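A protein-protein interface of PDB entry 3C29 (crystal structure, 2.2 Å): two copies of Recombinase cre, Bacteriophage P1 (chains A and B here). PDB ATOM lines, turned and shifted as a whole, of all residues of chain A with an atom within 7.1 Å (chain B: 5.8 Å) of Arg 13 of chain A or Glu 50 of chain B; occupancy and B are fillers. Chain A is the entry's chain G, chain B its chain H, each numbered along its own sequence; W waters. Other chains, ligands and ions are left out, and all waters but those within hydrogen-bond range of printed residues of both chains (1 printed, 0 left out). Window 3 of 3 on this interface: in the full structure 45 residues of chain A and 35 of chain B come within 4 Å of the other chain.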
ATOM      1  N   LYS A   6      -0.898  20.976 -35.042  1.00  0.00           N
ATOM      2  CA  LYS A   6      -0.850  21.662 -33.759  1.00  0.00           C
ATOM      3  C   LYS A   6      -2.154  22.439 -33.491  1.00  0.00           C
ATOM      4  O   LYS A   6      -2.745  22.325 -32.413  1.00  0.00           O
ATOM      5  CB  LYS A   6       0.384  22.574 -33.696  1.00  0.00           C
ATOM      6  CG  LYS A   6       0.717  23.089 -32.307  1.00  0.00           C
ATOM      7  CD  LYS A   6       0.111  24.466 -32.051  1.00  0.00           C
ATOM      8  CE  LYS A   6       0.921  25.256 -31.008  1.00  0.00           C
ATOM      9  NZ  LYS A   6       1.220  24.438 -29.787  1.00  0.00           N
ATOM     10  N   LEU A   8      -5.149  21.942 -34.651  1.00  0.00           N
ATOM     11  CA  LEU A   8      -6.241  21.014 -34.361  1.00  0.00           C
ATOM     12  C   LEU A   8      -6.103  20.357 -32.996  1.00  0.00           C
ATOM     13  O   LEU A   8      -7.117  20.079 -32.338  1.00  0.00           O
ATOM     14  CB  LEU A   8      -6.380  19.954 -35.451  1.00  0.00           C
ATOM     15  CG  LEU A   8      -6.703  20.402 -36.886  1.00  0.00           C
ATOM     16  CD1 LEU A   8      -6.443  19.256 -37.857  1.00  0.00           C
ATOM     17  CD2 LEU A   8      -8.120  20.962 -37.059  1.00  0.00           C
ATOM     18  N   MET A   9      -4.869  20.097 -32.568  1.00  0.00           N
ATOM     19  CA  MET A   9      -4.649  19.615 -31.198  1.00  0.00           C
ATOM     20  C   MET A   9      -5.090  20.654 -30.140  1.00  0.00           C
ATOM     21  O   MET A   9      -5.668  20.292 -29.123  1.00  0.00           O
ATOM     22  CB  MET A   9      -3.205  19.152 -30.985  1.00  0.00           C
ATOM     23  CG  MET A   9      -2.934  17.736 -31.549  1.00  0.00           C
ATOM     24  SD  MET A   9      -1.168  17.302 -31.800  1.00  0.00           S
ATOM     25  CE  MET A   9      -1.313  15.675 -32.602  1.00  0.00           C
ATOM     26  N   ASP A  10      -4.851  21.933 -30.418  1.00  0.00           N
ATOM     27  CA  ASP A  10      -5.346  23.024 -29.569  1.00  0.00           C
ATOM     28  C   ASP A  10      -6.881  22.996 -29.459  1.00  0.00           C
ATOM     29  O   ASP A  10      -7.434  23.200 -28.387  1.00  0.00           O
ATOM     30  CB  ASP A  10      -4.870  24.394 -30.099  1.00  0.00           C
ATOM     31  CG  ASP A  10      -3.357  24.619 -29.922  1.00  0.00           C
ATOM     32  OD1 ASP A  10      -2.672  23.816 -29.227  1.00  0.00           O
ATOM     33  OD2 ASP A  10      -2.850  25.614 -30.493  1.00  0.00           O
ATOM     34  N   MET A  11      -7.543  22.723 -30.578  1.00  0.00           N
ATOM     35  CA  MET A  11      -9.007  22.659 -30.662  1.00  0.00           C
ATOM     36  C   MET A  11      -9.580  21.535 -29.849  1.00  0.00           C
ATOM     37  O   MET A  11     -10.604  21.694 -29.198  1.00  0.00           O
ATOM     38  CB  MET A  11      -9.429  22.459 -32.109  1.00  0.00           C
ATOM     39  CG  MET A  11      -9.311  23.690 -32.925  1.00  0.00           C
ATOM     40  SD  MET A  11     -10.958  24.397 -33.026  1.00  0.00           S
ATOM     41  CE  MET A  11     -11.623  23.371 -34.348  1.00  0.00           C
ATOM     42  N   PHE A  12      -8.933  20.381 -29.907  1.00  0.00           N
ATOM     43  CA  PHE A  12      -9.336  19.287 -29.049  1.00  0.00           C
ATOM     44  C   PHE A  12      -9.084  19.601 -27.566  1.00  0.00           C
ATOM     45  O   PHE A  12      -9.969  19.439 -26.742  1.00  0.00           O
ATOM     46  CB  PHE A  12      -8.652  17.969 -29.441  1.00  0.00           C
ATOM     47  CG  PHE A  12      -9.053  16.823 -28.552  1.00  0.00           C
ATOM     48  CD1 PHE A  12      -8.261  16.458 -27.464  1.00  0.00           C
ATOM     49  CD2 PHE A  12     -10.265  16.150 -28.765  1.00  0.00           C
ATOM     50  CE1 PHE A  12      -8.649  15.419 -26.608  1.00  0.00           C
ATOM     51  CE2 PHE A  12     -10.666  15.111 -27.914  1.00  0.00           C
ATOM     52  CZ  PHE A  12      -9.853  14.745 -26.835  1.00  0.00           C
ATOM     53  N   ARG A  13      -7.875  20.041 -27.229  1.00  0.00           N
ATOM     54  CA  ARG A  13      -7.560  20.340 -25.849  1.00  0.00           C
ATOM     55  C   ARG A  13      -8.610  21.275 -25.244  1.00  0.00           C
ATOM     56  O   ARG A  13      -9.087  21.020 -24.153  1.00  0.00           O
ATOM     57  CB  ARG A  13      -6.152  20.934 -25.708  1.00  0.00           C
ATOM     58  CG  ARG A  13      -5.820  21.393 -24.279  1.00  0.00           C
ATOM     59  CD  ARG A  13      -4.403  21.948 -24.153  1.00  0.00           C
ATOM     60  NE  ARG A  13      -4.162  23.163 -24.922  1.00  0.00           N
ATOM     61  CZ  ARG A  13      -3.017  23.838 -24.910  1.00  0.00           C
ATOM     62  NH1 ARG A  13      -1.990  23.424 -24.169  1.00  0.00           N
ATOM     63  NH2 ARG A  13      -2.886  24.927 -25.659  1.00  0.00           N
ATOM     64  N   ASP A  14      -8.977  22.338 -25.958  1.00  0.00           N
ATOM     65  CA  ASP A  14      -9.947  23.294 -25.444  1.00  0.00           C
ATOM     66  C   ASP A  14     -11.313  23.175 -26.141  1.00  0.00           C
ATOM     67  O   ASP A  14     -11.945  24.193 -26.504  1.00  0.00           O
ATOM     68  CB  ASP A  14      -9.402  24.728 -25.541  1.00  0.00           C
ATOM     69  CG  ASP A  14      -8.397  25.066 -24.436  1.00  0.00           C
ATOM     70  OD1 ASP A  14      -8.565  24.603 -23.281  1.00  0.00           O
ATOM     71  OD2 ASP A  14      -7.425  25.786 -24.733  1.00  0.00           O
ATOM     72  N   ARG A  15     -11.775  21.937 -26.320  1.00  0.00           N
ATOM     73  CA  ARG A  15     -13.030  21.695 -27.045  1.00  0.00           C
ATOM     74  C   ARG A  15     -14.257  22.331 -26.375  1.00  0.00           C
ATOM     75  O   ARG A  15     -15.235  22.675 -27.048  1.00  0.00           O
ATOM     76  CB  ARG A  15     -13.239  20.199 -27.291  1.00  0.00           C
ATOM     77  CG  ARG A  15     -13.331  19.364 -26.040  1.00  0.00           C
ATOM     78  CD  ARG A  15     -13.002  17.906 -26.343  1.00  0.00           C
ATOM     79  NE  ARG A  15     -12.956  17.101 -25.118  1.00  0.00           N
ATOM     80  CZ  ARG A  15     -11.880  16.962 -24.340  1.00  0.00           C
ATOM     81  NH1 ARG A  15     -10.727  17.569 -24.642  1.00  0.00           N
ATOM     82  NH2 ARG A  15     -11.956  16.202 -23.253  1.00  0.00           N
ATOM     83  N   GLN A  16     -14.194  22.504 -25.057  1.00  0.00           N
ATOM     84  CA  GLN A  16     -15.255  23.174 -24.308  1.00  0.00           C
ATOM     85  C   GLN A  16     -15.353  24.660 -24.649  1.00  0.00           C
ATOM     86  O   GLN A  16     -16.208  25.342 -24.105  1.00  0.00           O
ATOM     87  CB  GLN A  16     -15.072  23.003 -22.799  1.00  0.00           C
ATOM     88  CG  GLN A  16     -15.420  21.631 -22.208  1.00  0.00           C
ATOM     89  CD  GLN A  16     -15.071  21.550 -20.698  1.00  0.00           C
ATOM     90  OE1 GLN A  16     -14.055  20.957 -20.321  1.00  0.00           O
ATOM     91  NE2 GLN A  16     -15.898  22.173 -19.845  1.00  0.00           N
ATOM     92  N   ALA A  17     -14.490  25.156 -25.540  1.00  0.00           N
ATOM     93  CA  ALA A  17     -14.659  26.476 -26.127  1.00  0.00           C
ATOM     94  C   ALA A  17     -15.937  26.576 -26.952  1.00  0.00           C
ATOM     95  O   ALA A  17     -16.414  27.662 -27.168  1.00  0.00           O
ATOM     96  CB  ALA A  17     -13.477  26.846 -27.007  1.00  0.00           C
ATOM     97  N   ARG B  42       8.208  32.214 -15.989  1.00  0.00           N
ATOM     98  CA  ARG B  42       7.881  32.522 -17.390  1.00  0.00           C
ATOM     99  C   ARG B  42       8.389  33.916 -17.743  1.00  0.00           C
ATOM    100  O   ARG B  42       8.595  34.742 -16.877  1.00  0.00           O
ATOM    101  CB  ARG B  42       6.363  32.460 -17.652  1.00  0.00           C
ATOM    102  CG  ARG B  42       5.580  31.348 -16.965  1.00  0.00           C
ATOM    103  CD  ARG B  42       5.983  29.925 -17.385  1.00  0.00           C
ATOM    104  NE  ARG B  42       5.253  28.975 -16.543  1.00  0.00           N
ATOM    105  CZ  ARG B  42       4.114  28.373 -16.878  1.00  0.00           C
ATOM    106  NH1 ARG B  42       3.561  28.573 -18.070  1.00  0.00           N
ATOM    107  NH2 ARG B  42       3.524  27.558 -16.005  1.00  0.00           N
ATOM    108  N   GLU B  48       4.228  34.401 -24.383  1.00  0.00           N
ATOM    109  CA  GLU B  48       3.991  33.145 -25.087  1.00  0.00           C
ATOM    110  C   GLU B  48       2.549  32.746 -24.912  1.00  0.00           C
ATOM    111  O   GLU B  48       2.035  32.778 -23.790  1.00  0.00           O
ATOM    112  CB  GLU B  48       4.804  32.025 -24.458  1.00  0.00           C
ATOM    113  CG  GLU B  48       5.800  31.398 -25.377  1.00  0.00           C
ATOM    114  CD  GLU B  48       6.793  32.403 -25.858  1.00  0.00           C
ATOM    115  OE1 GLU B  48       7.410  33.043 -24.981  1.00  0.00           O
ATOM    116  OE2 GLU B  48       6.936  32.561 -27.098  1.00  0.00           O
ATOM    117  N   PRO B  49       1.903  32.320 -26.001  1.00  0.00           N
ATOM    118  CA  PRO B  49       0.519  31.804 -25.954  1.00  0.00           C
ATOM    119  C   PRO B  49       0.286  30.756 -24.857  1.00  0.00           C
ATOM    120  O   PRO B  49      -0.642  30.903 -24.085  1.00  0.00           O
ATOM    121  CB  PRO B  49       0.320  31.213 -27.345  1.00  0.00           C
ATOM    122  CG  PRO B  49       1.236  32.049 -28.226  1.00  0.00           C
ATOM    123  CD  PRO B  49       2.458  32.314 -27.370  1.00  0.00           C
ATOM    124  N   GLU B  50       1.146  29.742 -24.767  1.00  0.00           N
ATOM    125  CA  GLU B  50       1.041  28.744 -23.703  1.00  0.00           C
ATOM    126  C   GLU B  50       1.104  29.351 -22.305  1.00  0.00           C
ATOM    127  O   GLU B  50       0.360  28.932 -21.452  1.00  0.00           O
ATOM    128  CB  GLU B  50       2.087  27.622 -23.868  1.00  0.00           C
ATOM    129  CG  GLU B  50       1.840  26.721 -25.091  1.00  0.00           C
ATOM    130  CD  GLU B  50       0.458  26.034 -25.049  1.00  0.00           C
ATOM    131  OE1 GLU B  50      -0.302  26.132 -26.042  1.00  0.00           O
ATOM    132  OE2 GLU B  50       0.118  25.410 -24.017  1.00  0.00           O
ATOM    133  N   ASP B  51       1.959  30.350 -22.083  1.00  0.00           N
ATOM    134  CA  ASP B  51       2.035  31.021 -20.784  1.00  0.00           C
ATOM    135  C   ASP B  51       0.777  31.857 -20.483  1.00  0.00           C
ATOM    136  O   ASP B  51       0.242  31.791 -19.380  1.00  0.00           O
ATOM    137  CB  ASP B  51       3.304  31.880 -20.678  1.00  0.00           C
ATOM    138  CG  ASP B  51       4.602  31.058 -20.792  1.00  0.00           C
ATOM    139  OD1 ASP B  51       4.613  29.863 -20.430  1.00  0.00           O
ATOM    140  OD2 ASP B  51       5.644  31.625 -21.201  1.00  0.00           O
ATOM    141  N   VAL B  52       0.321  32.644 -21.466  1.00  0.00           N
ATOM    142  CA  VAL B  52      -0.916  33.411 -21.316  1.00  0.00           C
ATOM    143  C   VAL B  52      -2.063  32.429 -21.031  1.00  0.00           C
ATOM    144  O   VAL B  52      -2.861  32.682 -20.119  1.00  0.00           O
ATOM    145  CB  VAL B  52      -1.223  34.285 -22.568  1.00  0.00           C
ATOM    146  CG1 VAL B  52      -2.519  35.035 -22.402  1.00  0.00           C
ATOM    147  CG2 VAL B  52      -0.090  35.263 -22.846  1.00  0.00           C
ATOM    148  N   ARG B  53      -2.112  31.298 -21.762  1.00  0.00           N
ATOM    149  CA  ARG B  53      -3.166  30.301 -21.518  1.00  0.00           C
ATOM    150  C   ARG B  53      -3.185  29.882 -20.029  1.00  0.00           C
ATOM    151  O   ARG B  53      -4.235  29.898 -19.415  1.00  0.00           O
ATOM    152  CB  ARG B  53      -3.099  29.051 -22.437  1.00  0.00           C
ATOM    153  CG  ARG B  53      -4.358  28.130 -22.243  1.00  0.00           C
ATOM    154  CD  ARG B  53      -4.531  26.854 -23.131  1.00  0.00           C
ATOM    155  NE  ARG B  53      -4.087  25.749 -22.286  1.00  0.00           N
ATOM    156  CZ  ARG B  53      -4.812  24.752 -21.817  1.00  0.00           C
ATOM    157  NH1 ARG B  53      -6.060  24.561 -22.175  1.00  0.00           N
ATOM    158  NH2 ARG B  53      -4.219  23.893 -21.008  1.00  0.00           N
ATOM    159  N   ASP B  54      -2.027  29.519 -19.476  1.00  0.00           N
ATOM    160  CA  ASP B  54      -1.922  29.126 -18.068  1.00  0.00           C
ATOM    161  C   ASP B  54      -2.339  30.231 -17.105  1.00  0.00           C
ATOM    162  O   ASP B  54      -3.016  29.970 -16.110  1.00  0.00           O
ATOM    163  CB  ASP B  54      -0.495  28.690 -17.735  1.00  0.00           C
ATOM    164  CG  ASP B  54      -0.125  27.373 -18.371  1.00  0.00           C
ATOM    165  OD1 ASP B  54      -1.034  26.623 -18.826  1.00  0.00           O
ATOM    166  OD2 ASP B  54       1.091  27.116 -18.467  1.00  0.00           O
ATOM    167  N   TYR B  55      -1.922  31.460 -17.400  1.00  0.00           N
ATOM    168  CA  TYR B  55      -2.309  32.603 -16.584  1.00  0.00           C
ATOM    169  C   TYR B  55      -3.850  32.751 -16.528  1.00  0.00           C
ATOM    170  O   TYR B  55      -4.412  32.928 -15.460  1.00  0.00           O
ATOM    171  CB  TYR B  55      -1.655  33.866 -17.128  1.00  0.00           C
ATOM    172  CG  TYR B  55      -2.060  35.167 -16.451  1.00  0.00           C
ATOM    173  CD1 TYR B  55      -1.751  35.418 -15.107  1.00  0.00           C
ATOM    174  CD2 TYR B  55      -2.725  36.159 -17.166  1.00  0.00           C
ATOM    175  CE1 TYR B  55      -2.098  36.606 -14.498  1.00  0.00           C
ATOM    176  CE2 TYR B  55      -3.064  37.379 -16.556  1.00  0.00           C
ATOM    177  CZ  TYR B  55      -2.740  37.585 -15.228  1.00  0.00           C
ATOM    178  OH  TYR B  55      -3.078  38.770 -14.630  1.00  0.00           O
ATOM    179  N   ALA B  93      -4.539  28.710 -28.746  1.00  0.00           N
ATOM    180  CA  ALA B  93      -4.445  28.287 -27.350  1.00  0.00           C
ATOM    181  C   ALA B  93      -5.085  29.335 -26.439  1.00  0.00           C
ATOM    182  O   ALA B  93      -5.726  29.007 -25.466  1.00  0.00           O
ATOM    183  CB  ALA B  93      -2.987  28.050 -26.951  1.00  0.00           C
ATOM    184  N   VAL B  94      -4.895  30.600 -26.775  1.00  0.00           N
ATOM    185  CA  VAL B  94      -5.433  31.683 -25.971  1.00  0.00           C
ATOM    186  C   VAL B  94      -6.871  31.987 -26.366  1.00  0.00           C
ATOM    187  O   VAL B  94      -7.741  32.104 -25.487  1.00  0.00           O
ATOM    188  CB  VAL B  94      -4.535  32.914 -26.050  1.00  0.00           C
ATOM    189  CG1 VAL B  94      -5.202  34.148 -25.453  1.00  0.00           C
ATOM    190  CG2 VAL B  94      -3.208  32.598 -25.339  1.00  0.00           C
ATOM    191  N   ARG B 100     -13.610  29.023 -23.696  1.00  0.00           N
ATOM    192  CA  ARG B 100     -13.883  27.947 -22.777  1.00  0.00           C
ATOM    193  C   ARG B 100     -14.176  28.440 -21.364  1.00  0.00           C
ATOM    194  O   ARG B 100     -15.108  27.997 -20.718  1.00  0.00           O
ATOM    195  CB  ARG B 100     -12.719  26.976 -22.794  1.00  0.00           C
ATOM    196  CG  ARG B 100     -12.776  25.965 -21.694  1.00  0.00           C
ATOM    197  CD  ARG B 100     -11.521  25.119 -21.739  1.00  0.00           C
ATOM    198  NE  ARG B 100     -11.600  24.068 -20.747  1.00  0.00           N
ATOM    199  CZ  ARG B 100     -10.624  23.196 -20.509  1.00  0.00           C
ATOM    200  NH1 ARG B 100      -9.487  23.261 -21.201  1.00  0.00           N
ATOM    201  NH2 ARG B 100     -10.801  22.248 -19.589  1.00  0.00           N
HETATM  202  O   HOH W   1       0.332  27.083 -28.378  1.00  0.00           O
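The side-chain carboxylate of Glu 50 of chain B lies within salt-bridge range of the guanidinium group of Arg 13 of chain A, 2.9 Å away. OD1 of Asp 14 of chain A is in salt-bridge range of NH1 of Arg 53 of chain B, 2.7 Å away. The guanidinium group (NH1) of Arg 100 of chain B lies within salt-bridge range of the side-chain carboxylate (OD1) of Asp 14 of chain A (2.6 Å).
The side-chain amino group of Lys 6 of chain A is in salt-bridge range of the side-chain carboxylate of Asp 10 of chain A (3.98 Å). The side-chain carboxylate (OD1) of Asp 10 of chain A is in salt-bridge range of the guanidinium group (NH2) of Arg 13 of chain A, 3.7 Å away.
Among the printed residues, pairs that only touch across the chains: Arg 13 of chain A with Ala 93 of chain B, Arg 13 of chain A with Arg 53 of chain B, Gln 16 of chain A with Arg 100 of chain B, Ala 17 of chain A with Arg 100 of chain B, Asp 14 of chain A with Ala 93 of chain B, Arg 13 of chain A with Arg 100 of chain B and Asp 10 of chain A with Ala 93 of chain B.
Of the printed residues of chain B, Asp 10 of chain A touches Ala 93 (3.9 Å). Arg 13 of chain A touches just these residues of chain B: Glu 50 (2.9 Å), Arg 53 (3.4 Å), Ala 93 (3.4 Å) and Arg 100 (3.7 Å). Of the printed residues of chain B, Asp 14 of chain A touches Arg 53, Ala 93 and Arg 100. Of the printed residues of chain B, Gln 16 of chain A touches Arg 100. Glu 50 of chain B touches just one residue of chain A: Arg 13. Of the printed residues of chain A, Arg 100 of chain B touches Arg 13 (3.7 Å), Asp 14 (2.6 Å), Gln 16 (3.6 Å) and Ala 17 (3.7 Å). The nearest printed residue of chain B that does not touch Arg 13 of chain A is Val 94 of chain B (6.1 Å). The nearest printed residue of chain B that does not touch Asp 10 of chain A is Glu 50 of chain B (4.6 Å).
Of the 12 printed residues of chain B, 4 touch a printed residue of chain A. Hydrophobic or aromatic side chains of chain B that line the printed part of chain A: Ala 93. Among the printed residues, 10 pairs touch across the chains.
No position is printed for both chains.
Water W1 bridges OE1 of Glu 50 of chain B and NZ of Lys 6 of chain A.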
